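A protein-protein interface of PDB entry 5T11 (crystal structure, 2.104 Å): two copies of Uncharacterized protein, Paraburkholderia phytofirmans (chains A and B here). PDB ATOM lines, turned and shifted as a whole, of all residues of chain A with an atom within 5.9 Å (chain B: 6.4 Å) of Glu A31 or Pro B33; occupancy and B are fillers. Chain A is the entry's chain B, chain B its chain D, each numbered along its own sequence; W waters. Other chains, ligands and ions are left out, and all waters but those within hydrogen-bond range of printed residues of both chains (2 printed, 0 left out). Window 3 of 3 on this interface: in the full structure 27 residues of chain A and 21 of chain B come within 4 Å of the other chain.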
ATOM      1  N   ASN A  28      20.585  18.616   0.961  1.00  0.00           N
ATOM      2  CA  ASN A  28      21.459  19.774   0.811  1.00  0.00           C
ATOM      3  C   ASN A  28      22.753  19.477   1.551  1.00  0.00           C
ATOM      4  O   ASN A  28      22.785  19.480   2.792  1.00  0.00           O
ATOM      5  CB  ASN A  28      20.791  21.056   1.323  1.00  0.00           C
ATOM      6  CG  ASN A  28      21.653  22.308   1.064  1.00  0.00           C
ATOM      7  OD1 ASN A  28      22.701  22.236   0.407  1.00  0.00           O
ATOM      8  ND2 ASN A  28      21.210  23.452   1.577  1.00  0.00           N
ATOM      9  N   TYR A  29      23.814  19.200   0.795  1.00  0.00           N
ATOM     10  CA  TYR A  29      25.118  18.951   1.392  1.00  0.00           C
ATOM     11  C   TYR A  29      26.035  20.161   1.307  1.00  0.00           C
ATOM     12  O   TYR A  29      27.237  20.039   1.545  1.00  0.00           O
ATOM     13  CB  TYR A  29      25.769  17.728   0.748  1.00  0.00           C
ATOM     14  CG  TYR A  29      24.969  16.460   0.977  1.00  0.00           C
ATOM     15  CD1 TYR A  29      24.256  16.268   2.159  1.00  0.00           C
ATOM     16  CD2 TYR A  29      24.903  15.460   0.002  1.00  0.00           C
ATOM     17  CE1 TYR A  29      23.512  15.107   2.367  1.00  0.00           C
ATOM     18  CE2 TYR A  29      24.159  14.303   0.210  1.00  0.00           C
ATOM     19  CZ  TYR A  29      23.470  14.142   1.389  1.00  0.00           C
ATOM     20  OH  TYR A  29      22.743  13.003   1.598  1.00  0.00           O
ATOM     21  N   THR A  30      25.495  21.321   0.974  1.00  0.00           N
ATOM     22  CA  THR A  30      26.268  22.546   0.918  1.00  0.00           C
ATOM     23  C   THR A  30      25.936  23.404   2.124  1.00  0.00           C
ATOM     24  O   THR A  30      25.020  23.124   2.900  1.00  0.00           O
ATOM     25  CB  THR A  30      25.956  23.331  -0.357  1.00  0.00           C
ATOM     26  OG1 THR A  30      24.746  24.086  -0.152  1.00  0.00           O
ATOM     27  CG2 THR A  30      25.758  22.367  -1.540  1.00  0.00           C
ATOM     28  N   GLU A  31      26.669  24.495   2.234  1.00  0.00           N
ATOM     29  CA  GLU A  31      26.424  25.507   3.242  1.00  0.00           C
ATOM     30  C   GLU A  31      25.597  26.660   2.692  1.00  0.00           C
ATOM     31  O   GLU A  31      25.497  27.695   3.340  1.00  0.00           O
ATOM     32  CB  GLU A  31      27.762  25.991   3.800  1.00  0.00           C
ATOM     33  CG  GLU A  31      28.465  24.874   4.565  1.00  0.00           C
ATOM     34  CD  GLU A  31      29.889  25.232   4.946  1.00  0.00           C
ATOM     35  OE1 GLU A  31      30.736  25.370   4.036  1.00  0.00           O
ATOM     36  OE2 GLU A  31      30.159  25.372   6.158  1.00  0.00           O
ATOM     37  N   THR A  32      24.995  26.503   1.511  1.00  0.00           N
ATOM     38  CA  THR A  32      24.041  27.487   1.018  1.00  0.00           C
ATOM     39  C   THR A  32      22.646  27.093   1.482  1.00  0.00           C
ATOM     40  O   THR A  32      22.133  26.049   1.047  1.00  0.00           O
ATOM     41  CB  THR A  32      24.096  27.581  -0.497  1.00  0.00           C
ATOM     42  OG1 THR A  32      25.440  27.879  -0.889  1.00  0.00           O
ATOM     43  CG2 THR A  32      23.174  28.696  -0.993  1.00  0.00           C
ATOM     44  N   PRO A  33      22.007  27.862   2.362  1.00  0.00           N
ATOM     45  CA  PRO A  33      20.673  27.479   2.839  1.00  0.00           C
ATOM     46  C   PRO A  33      19.703  27.314   1.680  1.00  0.00           C
ATOM     47  O   PRO A  33      19.734  28.074   0.712  1.00  0.00           O
ATOM     48  CB  PRO A  33      20.259  28.646   3.748  1.00  0.00           C
ATOM     49  CG  PRO A  33      21.573  29.334   4.154  1.00  0.00           C
ATOM     50  CD  PRO A  33      22.489  29.128   2.950  1.00  0.00           C
ATOM     51  N   ARG A 100      27.442  27.232  -4.823  1.00  0.00           N
ATOM     52  CA  ARG A 100      28.007  28.426  -4.195  1.00  0.00           C
ATOM     53  C   ARG A 100      28.736  29.228  -5.258  1.00  0.00           C
ATOM     54  O   ARG A 100      28.990  28.740  -6.365  1.00  0.00           O
ATOM     55  CB  ARG A 100      28.972  28.052  -3.061  1.00  0.00           C
ATOM     56  CG  ARG A 100      30.199  27.250  -3.562  1.00  0.00           C
ATOM     57  CD  ARG A 100      31.260  27.043  -2.478  1.00  0.00           C
ATOM     58  NE  ARG A 100      31.805  28.326  -2.008  1.00  0.00           N
ATOM     59  CZ  ARG A 100      32.846  28.440  -1.191  1.00  0.00           C
ATOM     60  NH1 ARG A 100      33.471  27.352  -0.735  1.00  0.00           N
ATOM     61  NH2 ARG A 100      33.269  29.640  -0.833  1.00  0.00           N
ATOM     62  N   ASN B  28      33.969  11.285   7.243  1.00  0.00           N
ATOM     63  CA  ASN B  28      34.390  12.631   6.836  1.00  0.00           C
ATOM     64  C   ASN B  28      35.523  13.070   7.758  1.00  0.00           C
ATOM     65  O   ASN B  28      35.279  13.546   8.869  1.00  0.00           O
ATOM     66  CB  ASN B  28      33.225  13.624   6.885  1.00  0.00           C
ATOM     67  CG  ASN B  28      33.604  15.006   6.353  1.00  0.00           C
ATOM     68  OD1 ASN B  28      34.721  15.219   5.877  1.00  0.00           O
ATOM     69  ND2 ASN B  28      32.662  15.952   6.422  1.00  0.00           N
ATOM     70  N   THR B  30      37.450  15.563   6.992  1.00  0.00           N
ATOM     71  CA  THR B  30      37.716  16.948   6.636  1.00  0.00           C
ATOM     72  C   THR B  30      36.880  17.868   7.523  1.00  0.00           C
ATOM     73  O   THR B  30      36.052  17.423   8.328  1.00  0.00           O
ATOM     74  CB  THR B  30      37.391  17.205   5.164  1.00  0.00           C
ATOM     75  OG1 THR B  30      35.983  17.454   5.041  1.00  0.00           O
ATOM     76  CG2 THR B  30      37.738  15.975   4.302  1.00  0.00           C
ATOM     77  N   GLU B  31      37.102  19.171   7.358  1.00  0.00           N
ATOM     78  CA  GLU B  31      36.260  20.199   7.951  1.00  0.00           C
ATOM     79  C   GLU B  31      35.251  20.770   6.954  1.00  0.00           C
ATOM     80  O   GLU B  31      34.734  21.868   7.163  1.00  0.00           O
ATOM     81  CB  GLU B  31      37.130  21.304   8.532  1.00  0.00           C
ATOM     82  CG  GLU B  31      37.910  20.843   9.749  1.00  0.00           C
ATOM     83  CD  GLU B  31      38.869  21.891  10.242  1.00  0.00           C
ATOM     84  OE1 GLU B  31      39.782  22.270   9.472  1.00  0.00           O
ATOM     85  OE2 GLU B  31      38.704  22.348  11.394  1.00  0.00           O
ATOM     86  N   THR B  32      34.966  20.056   5.867  1.00  0.00           N
ATOM     87  CA  THR B  32      33.874  20.460   4.998  1.00  0.00           C
ATOM     88  C   THR B  32      32.632  19.688   5.423  1.00  0.00           C
ATOM     89  O   THR B  32      32.611  18.457   5.287  1.00  0.00           O
ATOM     90  CB  THR B  32      34.207  20.201   3.541  1.00  0.00           C
ATOM     91  OG1 THR B  32      35.291  21.062   3.157  1.00  0.00           O
ATOM     92  CG2 THR B  32      32.995  20.506   2.657  1.00  0.00           C
ATOM     93  N   PRO B  33      31.616  20.345   5.992  1.00  0.00           N
ATOM     94  CA  PRO B  33      30.402  19.621   6.407  1.00  0.00           C
ATOM     95  C   PRO B  33      29.825  18.795   5.262  1.00  0.00           C
ATOM     96  O   PRO B  33      29.839  19.218   4.106  1.00  0.00           O
ATOM     97  CB  PRO B  33      29.442  20.745   6.836  1.00  0.00           C
ATOM     98  CG  PRO B  33      30.358  21.898   7.263  1.00  0.00           C
ATOM     99  CD  PRO B  33      31.585  21.777   6.356  1.00  0.00           C
ATOM    100  N   ASP B  34      29.353  17.590   5.598  1.00  0.00           N
ATOM    101  CA  ASP B  34      28.664  16.638   4.720  1.00  0.00           C
ATOM    102  C   ASP B  34      29.506  16.097   3.575  1.00  0.00           C
ATOM    103  O   ASP B  34      28.948  15.441   2.669  1.00  0.00           O
ATOM    104  CB  ASP B  34      27.382  17.231   4.126  1.00  0.00           C
ATOM    105  CG  ASP B  34      26.365  17.532   5.179  1.00  0.00           C
ATOM    106  OD1 ASP B  34      26.157  16.664   6.051  1.00  0.00           O
ATOM    107  OD2 ASP B  34      25.804  18.642   5.157  1.00  0.00           O
ATOM    108  N   ALA B  35      30.820  16.329   3.576  1.00  0.00           N
ATOM    109  CA  ALA B  35      31.631  15.843   2.467  1.00  0.00           C
ATOM    110  C   ALA B  35      31.533  14.332   2.323  1.00  0.00           C
ATOM    111  O   ALA B  35      31.613  13.815   1.206  1.00  0.00           O
ATOM    112  CB  ALA B  35      33.092  16.267   2.641  1.00  0.00           C
ATOM    113  N   GLY B  36      31.385  13.606   3.430  1.00  0.00           N
ATOM    114  CA  GLY B  36      31.205  12.170   3.324  1.00  0.00           C
ATOM    115  C   GLY B  36      29.893  11.808   2.654  1.00  0.00           C
ATOM    116  O   GLY B  36      29.838  10.890   1.829  1.00  0.00           O
ATOM    117  N   HIS B  37      28.820  12.531   2.980  1.00  0.00           N
ATOM    118  CA  HIS B  37      27.525  12.245   2.359  1.00  0.00           C
ATOM    119  C   HIS B  37      27.554  12.545   0.865  1.00  0.00           C
ATOM    120  O   HIS B  37      26.950  11.815   0.062  1.00  0.00           O
ATOM    121  CB  HIS B  37      26.425  13.050   3.050  1.00  0.00           C
ATOM    122  CG  HIS B  37      26.241  12.692   4.489  1.00  0.00           C
ATOM    123  ND1 HIS B  37      26.315  13.620   5.505  1.00  0.00           N
ATOM    124  CD2 HIS B  37      25.988  11.503   5.084  1.00  0.00           C
ATOM    125  CE1 HIS B  37      26.106  13.021   6.664  1.00  0.00           C
ATOM    126  NE2 HIS B  37      25.906  11.736   6.436  1.00  0.00           N
ATOM    127  N   SER B  38      28.258  13.613   0.478  1.00  0.00           N
ATOM    128  CA  SER B  38      28.463  13.914  -0.933  1.00  0.00           C
ATOM    129  C   SER B  38      29.197  12.786  -1.620  1.00  0.00           C
ATOM    130  O   SER B  38      28.788  12.334  -2.695  1.00  0.00           O
ATOM    131  CB  SER B  38      29.235  15.229  -1.092  1.00  0.00           C
ATOM    132  OG  SER B  38      28.392  16.283  -0.678  1.00  0.00           O
HETATM  133  O   HOH W   1      24.365  10.291   1.171  1.00  0.00           O
HETATM  134  O   HOH W   2      29.191  21.593   3.118  1.00  0.00           O
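Of the 10 printed residues of chain B, 4 touch a printed residue of chain A.
Hydrophobic or aromatic side chains of chain B within 4 Å of the printed part of chain A: Pro B33 and His B37.
Among the printed residues, 6 pairs touch across the chains.
Glu A31 touches just one residue of chain B: Pro B33.
Of chain A, only Tyr A29 (3.7 Å) and Glu A31 (3.7 Å) come within 4 Å of Pro B33.
Of the printed residues of chain A, Ser B38 touches Tyr A29.
Printed residues of chain B within 4 Å of Tyr A29: Pro B33, Asp B34, His B37 and Ser B38.
Arg A100 touches none of the printed residues of chain B.
Thr B32 touches none of the printed residues of chain A.
OD1 of Asp B34 lies within hydrogen-bond range of ND1 of His B37.
The side-chain amide nitrogen (ND2) of Asn A28 sits at hydrogen-bond distance from the backbone carbonyl oxygen (O) of Thr A32.
The side-chain amide oxygen of Asn A28 sits at hydrogen-bond distance from the side-chain hydroxyl of Thr A30, at 2.8 Å.
The backbone carbonyl oxygen (O) of Asp B34 is in hydrogen-bond range of the side-chain hydroxyl (OG) of Ser B38, at 3.5 Å.
Water W2 lies within hydrogen-bond range of O of Pro B33 and O of Tyr A29.
Water W1 lies within hydrogen-bond range of the side-chain hydroxyl of Tyr A29 (3.2 Å) and the backbone carbonyl oxygen of His B37 (3.2 Å).
Glu A31 touches Pro B33, but with the chains exchanged Pro A33 does not touch Glu B31 (14.8 Å).
Asn A28 touches Asp B34 (O to OD2, 3.9 Å).
Tyr A29 touches Pro B33.
Tyr A29 touches Asp B34.
CB of His B37 touches CZ of Tyr A29, 3.6 Å away.
CB of Tyr A29 touches OG of Ser B38, 3.3 Å away.
Glu A31 touches Pro B33.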
